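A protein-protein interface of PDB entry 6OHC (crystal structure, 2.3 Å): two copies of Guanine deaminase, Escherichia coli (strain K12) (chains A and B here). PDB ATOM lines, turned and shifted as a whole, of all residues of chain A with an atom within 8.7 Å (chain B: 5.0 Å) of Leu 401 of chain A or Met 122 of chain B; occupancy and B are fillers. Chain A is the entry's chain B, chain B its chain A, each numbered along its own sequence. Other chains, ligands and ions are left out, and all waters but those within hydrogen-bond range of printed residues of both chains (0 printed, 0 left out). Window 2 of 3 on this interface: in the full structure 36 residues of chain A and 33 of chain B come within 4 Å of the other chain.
The backbone carbonyl oxygen (O) of Ser 88 of chain B lies within hydrogen-bond range of the guanidinium group (NH1) of Arg 402 of chain A, at 3.1 Å.
The backbone carbonyl oxygen (O) of Arg 402 of chain A sits at hydrogen-bond distance from the side-chain hydroxyl (OG) of Ser 406 of chain A (2.7 Å).
OE2 of Glu 89 of chain B lies within hydrogen-bond range of OH of Tyr 118 of chain B (2.4 Å).
OE1 of Glu 89 of chain B lies within hydrogen-bond range of OH of Tyr 113 of chain B.
Among the printed residues, pairs that only touch across the chains: Leu 401 of chain A with Met 122 of chain B, Leu 398 of chain A with Ser 88 of chain B, Leu 401 of chain A with Phe 125 of chain B, Leu 401 of chain A with Glu 89 of chain B, Asn 405 of chain A with Glu 89 of chain B and Leu 401 of chain A with Ser 88 of chain B.
Of the printed residues of chain B, Leu 398 of chain A touches Ser 88.
Gln 399 of chain A touches none of the printed residues of chain B.
Of chain B, only Ser 88, Glu 89, Met 122 and Phe 125 come within 4 Å of Leu 401 of chain A.
Of the printed residues of chain B, Arg 402 of chain A touches Ser 88 (3.1 Å).
Of the printed residues of chain B, Asn 405 of chain A touches Glu 89.
Of the printed residues of chain A, Glu 89 of chain B touches Leu 401 and Asn 405.
Met 122 of chain B touches one residue of chain A.
Of the 14 printed residues of chain B, 4 touch a printed residue of chain A.
Of the 16 printed residues of chain A, 4 touch a printed residue of chain B.
Hydrophobic or aromatic side chains of chain A within 4 Å of the printed part of chain B: Leu 398 and Leu 401.
Along chain A the printed residues that touch a printed residue of chain B span positions 398 to 405.
Among the printed residues, 7 pairs touch across the chains.
No position is printed for both chains.
Of the 7 pairs that touch across the chains among the printed residues, none has its exchanged pair printed and touching as well.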
ATOM      1  N   PRO A 393      -6.777  27.116  36.429  1.00  0.00           N
ATOM      2  CA  PRO A 393      -5.542  26.398  36.145  1.00  0.00           C
ATOM      3  C   PRO A 393      -4.505  27.264  35.417  1.00  0.00           C
ATOM      4  O   PRO A 393      -3.377  26.776  35.239  1.00  0.00           O
ATOM      5  CB  PRO A 393      -6.050  25.255  35.240  1.00  0.00           C
ATOM      6  CG  PRO A 393      -7.178  25.884  34.489  1.00  0.00           C
ATOM      7  CD  PRO A 393      -7.876  26.715  35.546  1.00  0.00           C
ATOM      8  N   THR A 394      -4.830  28.540  35.133  1.00  0.00           N
ATOM      9  CA  THR A 394      -3.903  29.516  34.501  1.00  0.00           C
ATOM     10  C   THR A 394      -3.436  30.572  35.515  1.00  0.00           C
ATOM     11  O   THR A 394      -2.993  31.664  35.069  1.00  0.00           O
ATOM     12  CB  THR A 394      -4.608  30.164  33.310  1.00  0.00           C
ATOM     13  OG1 THR A 394      -5.760  30.864  33.774  1.00  0.00           O
ATOM     14  CG2 THR A 394      -5.099  29.155  32.295  1.00  0.00           C
ATOM     15  N   ALA A 395      -3.513  30.234  36.823  1.00  0.00           N
ATOM     16  CA  ALA A 395      -3.307  31.157  37.964  1.00  0.00           C
ATOM     17  C   ALA A 395      -1.873  31.718  37.980  1.00  0.00           C
ATOM     18  O   ALA A 395      -1.772  32.892  38.257  1.00  0.00           O
ATOM     19  CB  ALA A 395      -3.678  30.491  39.270  1.00  0.00           C
ATOM     20  N   THR A 396      -0.832  30.973  37.583  1.00  0.00           N
ATOM     21  CA  THR A 396       0.574  31.497  37.463  1.00  0.00           C
ATOM     22  C   THR A 396       0.985  31.566  35.999  1.00  0.00           C
ATOM     23  O   THR A 396       0.371  30.957  35.148  1.00  0.00           O
ATOM     24  CB  THR A 396       1.551  30.670  38.311  1.00  0.00           C
ATOM     25  OG1 THR A 396       1.704  29.341  37.804  1.00  0.00           O
ATOM     26  CG2 THR A 396       1.086  30.522  39.758  1.00  0.00           C
ATOM     27  N   PRO A 397       1.973  32.398  35.643  1.00  0.00           N
ATOM     28  CA  PRO A 397       2.377  32.508  34.261  1.00  0.00           C
ATOM     29  C   PRO A 397       2.903  31.179  33.728  1.00  0.00           C
ATOM     30  O   PRO A 397       2.654  30.893  32.579  1.00  0.00           O
ATOM     31  CB  PRO A 397       3.366  33.665  34.256  1.00  0.00           C
ATOM     32  CG  PRO A 397       2.973  34.487  35.454  1.00  0.00           C
ATOM     33  CD  PRO A 397       2.594  33.436  36.485  1.00  0.00           C
ATOM     34  N   LEU A 398       3.558  30.354  34.539  1.00  0.00           N
ATOM     35  CA  LEU A 398       4.073  29.040  34.040  1.00  0.00           C
ATOM     36  C   LEU A 398       2.891  28.108  33.799  1.00  0.00           C
ATOM     37  O   LEU A 398       2.902  27.369  32.798  1.00  0.00           O
ATOM     38  CB  LEU A 398       5.086  28.451  35.007  1.00  0.00           C
ATOM     39  CG  LEU A 398       5.645  27.077  34.652  1.00  0.00           C
ATOM     40  CD1 LEU A 398       6.481  27.138  33.375  1.00  0.00           C
ATOM     41  CD2 LEU A 398       6.503  26.558  35.796  1.00  0.00           C
ATOM     42  N   GLN A 399       1.894  28.159  34.673  1.00  0.00           N
ATOM     43  CA  GLN A 399       0.672  27.365  34.481  1.00  0.00           C
ATOM     44  C   GLN A 399      -0.061  27.828  33.211  1.00  0.00           C
ATOM     45  O   GLN A 399      -0.610  26.964  32.542  1.00  0.00           O
ATOM     46  CB  GLN A 399      -0.229  27.400  35.723  1.00  0.00           C
ATOM     47  CG  GLN A 399       0.367  26.576  36.865  1.00  0.00           C
ATOM     48  CD  GLN A 399       0.423  25.073  36.627  1.00  0.00           C
ATOM     49  OE1 GLN A 399      -0.548  24.351  36.960  1.00  0.00           O
ATOM     50  NE2 GLN A 399       1.578  24.560  36.157  1.00  0.00           N
ATOM     51  N   GLN A 400      -0.181  29.129  32.967  1.00  0.00           N
ATOM     52  CA  GLN A 400      -0.893  29.675  31.788  1.00  0.00           C
ATOM     53  C   GLN A 400      -0.157  29.150  30.545  1.00  0.00           C
ATOM     54  O   GLN A 400      -0.853  28.568  29.655  1.00  0.00           O
ATOM     55  CB  GLN A 400      -1.001  31.204  31.885  1.00  0.00           C
ATOM     56  CG  GLN A 400      -1.285  31.946  30.584  1.00  0.00           C
ATOM     57  CD  GLN A 400      -2.755  32.150  30.353  1.00  0.00           C
ATOM     58  OE1 GLN A 400      -3.459  32.680  31.200  1.00  0.00           O
ATOM     59  NE2 GLN A 400      -3.273  31.678  29.233  1.00  0.00           N
ATOM     60  N   LEU A 401       1.184  29.266  30.547  1.00  0.00           N
ATOM     61  CA  LEU A 401       2.029  28.770  29.453  1.00  0.00           C
ATOM     62  C   LEU A 401       1.714  27.289  29.229  1.00  0.00           C
ATOM     63  O   LEU A 401       1.458  26.945  28.084  1.00  0.00           O
ATOM     64  CB  LEU A 401       3.512  28.985  29.798  1.00  0.00           C
ATOM     65  CG  LEU A 401       4.532  28.489  28.772  1.00  0.00           C
ATOM     66  CD1 LEU A 401       4.435  29.270  27.469  1.00  0.00           C
ATOM     67  CD2 LEU A 401       5.945  28.644  29.303  1.00  0.00           C
ATOM     68  N   ARG A 402       1.767  26.443  30.259  1.00  0.00           N
ATOM     69  CA  ARG A 402       1.716  24.983  30.047  1.00  0.00           C
ATOM     70  C   ARG A 402       0.303  24.609  29.593  1.00  0.00           C
ATOM     71  O   ARG A 402       0.160  23.687  28.762  1.00  0.00           O
ATOM     72  CB  ARG A 402       2.109  24.169  31.283  1.00  0.00           C
ATOM     73  CG  ARG A 402       3.382  24.576  32.024  1.00  0.00           C
ATOM     74  CD  ARG A 402       4.169  23.377  32.534  1.00  0.00           C
ATOM     75  NE  ARG A 402       4.741  23.431  33.872  1.00  0.00           N
ATOM     76  CZ  ARG A 402       6.038  23.320  34.155  1.00  0.00           C
ATOM     77  NH1 ARG A 402       6.958  23.191  33.194  1.00  0.00           N
ATOM     78  NH2 ARG A 402       6.409  23.318  35.422  1.00  0.00           N
ATOM     79  N   TYR A 403      -0.716  25.316  30.074  1.00  0.00           N
ATOM     80  CA  TYR A 403      -2.128  24.959  29.792  1.00  0.00           C
ATOM     81  C   TYR A 403      -2.397  25.326  28.333  1.00  0.00           C
ATOM     82  O   TYR A 403      -2.854  24.465  27.638  1.00  0.00           O
ATOM     83  CB  TYR A 403      -3.065  25.683  30.747  1.00  0.00           C
ATOM     84  CG  TYR A 403      -4.454  25.129  30.860  1.00  0.00           C
ATOM     85  CD1 TYR A 403      -4.738  24.103  31.741  1.00  0.00           C
ATOM     86  CD2 TYR A 403      -5.533  25.770  30.269  1.00  0.00           C
ATOM     87  CE1 TYR A 403      -6.035  23.633  31.909  1.00  0.00           C
ATOM     88  CE2 TYR A 403      -6.842  25.369  30.492  1.00  0.00           C
ATOM     89  CZ  TYR A 403      -7.091  24.279  31.291  1.00  0.00           C
ATOM     90  OH  TYR A 403      -8.369  23.813  31.444  1.00  0.00           O
ATOM     91  N   ASP A 404      -2.064  26.560  27.943  1.00  0.00           N
ATOM     92  CA  ASP A 404      -2.074  27.048  26.546  1.00  0.00           C
ATOM     93  C   ASP A 404      -1.394  26.032  25.612  1.00  0.00           C
ATOM     94  O   ASP A 404      -1.803  25.949  24.471  1.00  0.00           O
ATOM     95  CB  ASP A 404      -1.317  28.365  26.343  1.00  0.00           C
ATOM     96  CG  ASP A 404      -2.016  29.609  26.865  1.00  0.00           C
ATOM     97  OD1 ASP A 404      -3.253  29.495  27.283  1.00  0.00           O
ATOM     98  OD2 ASP A 404      -1.260  30.713  26.855  1.00  0.00           O
ATOM     99  N   ASN A 405      -0.346  25.346  26.046  1.00  0.00           N
ATOM    100  CA  ASN A 405       0.470  24.510  25.142  1.00  0.00           C
ATOM    101  C   ASN A 405      -0.056  23.089  25.115  1.00  0.00           C
ATOM    102  O   ASN A 405       0.295  22.402  24.159  1.00  0.00           O
ATOM    103  CB  ASN A 405       1.929  24.499  25.522  1.00  0.00           C
ATOM    104  CG  ASN A 405       2.840  24.416  24.323  1.00  0.00           C
ATOM    105  OD1 ASN A 405       3.094  25.438  23.664  1.00  0.00           O
ATOM    106  ND2 ASN A 405       3.403  23.225  24.112  1.00  0.00           N
ATOM    107  N   SER A 406      -0.983  22.762  25.996  1.00  0.00           N
ATOM    108  CA  SER A 406      -1.714  21.485  26.034  1.00  0.00           C
ATOM    109  C   SER A 406      -2.864  21.499  25.026  1.00  0.00           C
ATOM    110  O   SER A 406      -3.693  22.429  25.133  1.00  0.00           O
ATOM    111  CB  SER A 406      -2.222  21.314  27.439  1.00  0.00           C
ATOM    112  OG  SER A 406      -1.128  21.299  28.331  1.00  0.00           O
ATOM    113  N   LYS A 412      -4.527  19.063  29.555  1.00  0.00           N
ATOM    114  CA  LYS A 412      -4.964  20.200  30.399  1.00  0.00           C
ATOM    115  C   LYS A 412      -5.303  19.690  31.804  1.00  0.00           C
ATOM    116  O   LYS A 412      -4.870  20.269  32.786  1.00  0.00           O
ATOM    117  CB  LYS A 412      -6.212  20.867  29.825  1.00  0.00           C
ATOM    118  CG  LYS A 412      -5.976  21.743  28.617  1.00  0.00           C
ATOM    119  CD  LYS A 412      -7.272  22.390  28.155  1.00  0.00           C
ATOM    120  CE  LYS A 412      -7.040  23.396  27.048  1.00  0.00           C
ATOM    121  NZ  LYS A 412      -5.959  22.938  26.138  1.00  0.00           N
ATOM    122  N   VAL A 415      -2.131  18.948  33.657  1.00  0.00           N
ATOM    123  CA  VAL A 415      -1.510  20.210  34.165  1.00  0.00           C
ATOM    124  C   VAL A 415      -2.349  20.738  35.367  1.00  0.00           C
ATOM    125  O   VAL A 415      -1.805  21.179  36.307  1.00  0.00           O
ATOM    126  CB  VAL A 415      -1.382  21.257  33.049  1.00  0.00           C
ATOM    127  CG1 VAL A 415      -1.016  22.650  33.557  1.00  0.00           C
ATOM    128  CG2 VAL A 415      -0.417  20.800  31.982  1.00  0.00           C
ATOM    129  N   TYR B  85      16.645  25.521  28.722  1.00  0.00           N
ATOM    130  CA  TYR B  85      15.908  26.786  28.442  1.00  0.00           C
ATOM    131  C   TYR B  85      14.736  26.555  27.500  1.00  0.00           C
ATOM    132  O   TYR B  85      13.677  27.138  27.677  1.00  0.00           O
ATOM    133  CB  TYR B  85      16.902  27.838  27.966  1.00  0.00           C
ATOM    134  CG  TYR B  85      16.557  28.612  26.728  1.00  0.00           C
ATOM    135  CD1 TYR B  85      15.486  29.499  26.716  1.00  0.00           C
ATOM    136  CD2 TYR B  85      17.338  28.498  25.586  1.00  0.00           C
ATOM    137  CE1 TYR B  85      15.221  30.279  25.607  1.00  0.00           C
ATOM    138  CE2 TYR B  85      17.046  29.248  24.462  1.00  0.00           C
ATOM    139  CZ  TYR B  85      16.010  30.148  24.480  1.00  0.00           C
ATOM    140  OH  TYR B  85      15.759  30.864  23.364  1.00  0.00           O
ATOM    141  N   SER B  88      10.481  25.184  28.917  1.00  0.00           N
ATOM    142  CA  SER B  88       9.554  25.836  29.861  1.00  0.00           C
ATOM    143  C   SER B  88       8.102  25.328  29.692  1.00  0.00           C
ATOM    144  O   SER B  88       7.484  24.962  30.730  1.00  0.00           O
ATOM    145  CB  SER B  88       9.646  27.322  29.764  1.00  0.00           C
ATOM    146  OG  SER B  88      10.888  27.791  30.223  1.00  0.00           O
ATOM    147  N   GLU B  89       7.603  25.213  28.456  1.00  0.00           N
ATOM    148  CA  GLU B  89       6.193  24.863  28.140  1.00  0.00           C
ATOM    149  C   GLU B  89       5.948  23.346  28.144  1.00  0.00           C
ATOM    150  O   GLU B  89       4.811  22.974  27.961  1.00  0.00           O
ATOM    151  CB  GLU B  89       5.775  25.432  26.784  1.00  0.00           C
ATOM    152  CG  GLU B  89       6.579  24.942  25.596  1.00  0.00           C
ATOM    153  CD  GLU B  89       7.780  25.810  25.187  1.00  0.00           C
ATOM    154  OE1 GLU B  89       8.611  26.071  26.041  1.00  0.00           O
ATOM    155  OE2 GLU B  89       7.865  26.242  24.029  1.00  0.00           O
ATOM    156  N   TYR B 113      11.815  26.526  18.860  1.00  0.00           N
ATOM    157  CA  TYR B 113      12.872  27.520  19.195  1.00  0.00           C
ATOM    158  C   TYR B 113      13.748  27.779  17.969  1.00  0.00           C
ATOM    159  O   TYR B 113      14.695  28.559  18.100  1.00  0.00           O
ATOM    160  CB  TYR B 113      13.635  27.122  20.462  1.00  0.00           C
ATOM    161  CG  TYR B 113      12.818  27.241  21.724  1.00  0.00           C
ATOM    162  CD1 TYR B 113      11.838  26.312  22.030  1.00  0.00           C
ATOM    163  CD2 TYR B 113      13.026  28.277  22.616  1.00  0.00           C
ATOM    164  CE1 TYR B 113      11.094  26.409  23.206  1.00  0.00           C
ATOM    165  CE2 TYR B 113      12.296  28.388  23.794  1.00  0.00           C
ATOM    166  CZ  TYR B 113      11.326  27.455  24.091  1.00  0.00           C
ATOM    167  OH  TYR B 113      10.589  27.557  25.226  1.00  0.00           O
ATOM    168  N   TYR B 118      10.159  33.637  18.750  1.00  0.00           N
ATOM    169  CA  TYR B 118       9.757  32.683  19.817  1.00  0.00           C
ATOM    170  C   TYR B 118      10.898  32.539  20.843  1.00  0.00           C
ATOM    171  O   TYR B 118      10.673  32.724  22.079  1.00  0.00           O
ATOM    172  CB  TYR B 118       9.396  31.301  19.277  1.00  0.00           C
ATOM    173  CG  TYR B 118       8.641  30.486  20.297  1.00  0.00           C
ATOM    174  CD1 TYR B 118       7.393  30.876  20.775  1.00  0.00           C
ATOM    175  CD2 TYR B 118       9.225  29.378  20.858  1.00  0.00           C
ATOM    176  CE1 TYR B 118       6.743  30.164  21.781  1.00  0.00           C
ATOM    177  CE2 TYR B 118       8.571  28.643  21.838  1.00  0.00           C
ATOM    178  CZ  TYR B 118       7.324  29.015  22.299  1.00  0.00           C
ATOM    179  OH  TYR B 118       6.745  28.276  23.296  1.00  0.00           O
ATOM    180  N   ALA B 119      12.114  32.303  20.337  1.00  0.00           N
ATOM    181  CA  ALA B 119      13.313  32.167  21.179  1.00  0.00           C
ATOM    182  C   ALA B 119      13.530  33.436  22.023  1.00  0.00           C
ATOM    183  O   ALA B 119      13.916  33.303  23.221  1.00  0.00           O
ATOM    184  CB  ALA B 119      14.486  31.817  20.337  1.00  0.00           C
ATOM    185  N   ARG B 120      13.258  34.606  21.450  1.00  0.00           N
ATOM    186  CA  ARG B 120      13.455  35.919  22.136  1.00  0.00           C
ATOM    187  C   ARG B 120      12.431  36.050  23.275  1.00  0.00           C
ATOM    188  O   ARG B 120      12.818  36.448  24.394  1.00  0.00           O
ATOM    189  CB  ARG B 120      13.307  37.078  21.145  1.00  0.00           C
ATOM    190  CG  ARG B 120      12.827  38.383  21.769  1.00  0.00           C
ATOM    191  CD  ARG B 120      12.594  39.486  20.755  1.00  0.00           C
ATOM    192  NE  ARG B 120      12.652  40.784  21.436  1.00  0.00           N
ATOM    193  CZ  ARG B 120      12.899  41.957  20.843  1.00  0.00           C
ATOM    194  NH1 ARG B 120      13.092  42.028  19.537  1.00  0.00           N
ATOM    195  NH2 ARG B 120      12.960  43.070  21.555  1.00  0.00           N
ATOM    196  N   GLU B 121      11.173  35.755  22.969  1.00  0.00           N
ATOM    197  CA  GLU B 121      10.049  35.863  23.923  1.00  0.00           C
ATOM    198  C   GLU B 121      10.334  34.901  25.082  1.00  0.00           C
ATOM    199  O   GLU B 121      10.315  35.353  26.208  1.00  0.00           O
ATOM    200  CB  GLU B 121       8.694  35.652  23.243  1.00  0.00           C
ATOM    201  CG  GLU B 121       7.578  36.165  24.163  1.00  0.00           C
ATOM    202  CD  GLU B 121       6.120  35.997  23.728  1.00  0.00           C
ATOM    203  OE1 GLU B 121       5.764  34.917  23.138  1.00  0.00           O
ATOM    204  OE2 GLU B 121       5.346  36.943  23.995  1.00  0.00           O
ATOM    205  N   MET B 122      10.710  33.658  24.766  1.00  0.00           N
ATOM    206  CA  MET B 122      10.937  32.572  25.732  1.00  0.00           C
ATOM    207  C   MET B 122      12.252  32.781  26.493  1.00  0.00           C
ATOM    208  O   MET B 122      12.299  32.391  27.712  1.00  0.00           O
ATOM    209  CB  MET B 122      10.891  31.205  25.048  1.00  0.00           C
ATOM    210  CG  MET B 122       9.481  30.797  24.631  1.00  0.00           C
ATOM    211  SD  MET B 122       8.104  31.260  25.803  1.00  0.00           S
ATOM    212  CE  MET B 122       8.288  29.889  26.938  1.00  0.00           C
ATOM    213  N   SER B 123      13.268  33.401  25.905  1.00  0.00           N
ATOM    214  CA  SER B 123      14.461  33.831  26.678  1.00  0.00           C
ATOM    215  C   SER B 123      14.054  34.771  27.824  1.00  0.00           C
ATOM    216  O   SER B 123      14.533  34.589  28.938  1.00  0.00           O
ATOM    217  CB  SER B 123      15.487  34.474  25.792  1.00  0.00           C
ATOM    218  OG  SER B 123      16.086  33.493  24.973  1.00  0.00           O
ATOM    219  N   ALA B 124      13.240  35.770  27.545  1.00  0.00           N
ATOM    220  CA  ALA B 124      12.779  36.738  28.572  1.00  0.00           C
ATOM    221  C   ALA B 124      11.954  36.005  29.668  1.00  0.00           C
ATOM    222  O   ALA B 124      12.132  36.263  30.858  1.00  0.00           O
ATOM    223  CB  ALA B 124      11.966  37.801  27.905  1.00  0.00           C
ATOM    224  N   PHE B 125      11.079  35.109  29.249  1.00  0.00           N
ATOM    225  CA  PHE B 125      10.245  34.298  30.144  1.00  0.00           C
ATOM    226  C   PHE B 125      11.166  33.399  30.999  1.00  0.00           C
ATOM    227  O   PHE B 125      10.968  33.286  32.226  1.00  0.00           O
ATOM    228  CB  PHE B 125       9.246  33.483  29.335  1.00  0.00           C
ATOM    229  CG  PHE B 125       8.414  32.609  30.214  1.00  0.00           C
ATOM    230  CD1 PHE B 125       7.240  33.090  30.765  1.00  0.00           C
ATOM    231  CD2 PHE B 125       8.815  31.322  30.515  1.00  0.00           C
ATOM    232  CE1 PHE B 125       6.507  32.311  31.638  1.00  0.00           C
ATOM    233  CE2 PHE B 125       8.090  30.565  31.430  1.00  0.00           C
ATOM    234  CZ  PHE B 125       6.947  31.059  31.986  1.00  0.00           C
ATOM    235  N   PHE B 126      12.169  32.791  30.384  1.00  0.00           N
ATOM    236  CA  PHE B 126      13.089  31.859  31.079  1.00  0.00           C
ATOM    237  C   PHE B 126      13.856  32.596  32.189  1.00  0.00           C
ATOM    238  O   PHE B 126      13.920  32.099  33.354  1.00  0.00           O
ATOM    239  CB  PHE B 126      14.005  31.154  30.093  1.00  0.00           C
ATOM    240  CG  PHE B 126      15.007  30.231  30.716  1.00  0.00           C
ATOM    241  CD1 PHE B 126      14.650  28.966  31.151  1.00  0.00           C
ATOM    242  CD2 PHE B 126      16.314  30.657  30.886  1.00  0.00           C
ATOM    243  CE1 PHE B 126      15.610  28.122  31.693  1.00  0.00           C
ATOM    244  CE2 PHE B 126      17.265  29.805  31.423  1.00  0.00           C
ATOM    245  CZ  PHE B 126      16.915  28.544  31.810  1.00  0.00           C
ATOM    246  N   ILE B 127      14.378  33.764  31.884  1.00  0.00           N
ATOM    247  CA  ILE B 127      15.194  34.538  32.854  1.00  0.00           C
ATOM    248  C   ILE B 127      14.272  35.012  33.992  1.00  0.00           C
ATOM    249  O   ILE B 127      14.668  34.901  35.142  1.00  0.00           O
ATOM    250  CB  ILE B 127      15.943  35.698  32.193  1.00  0.00           C
ATOM    251  CG1 ILE B 127      16.881  35.207  31.082  1.00  0.00           C
ATOM    252  CG2 ILE B 127      16.673  36.485  33.249  1.00  0.00           C
ATOM    253  CD1 ILE B 127      18.052  34.405  31.574  1.00  0.00           C
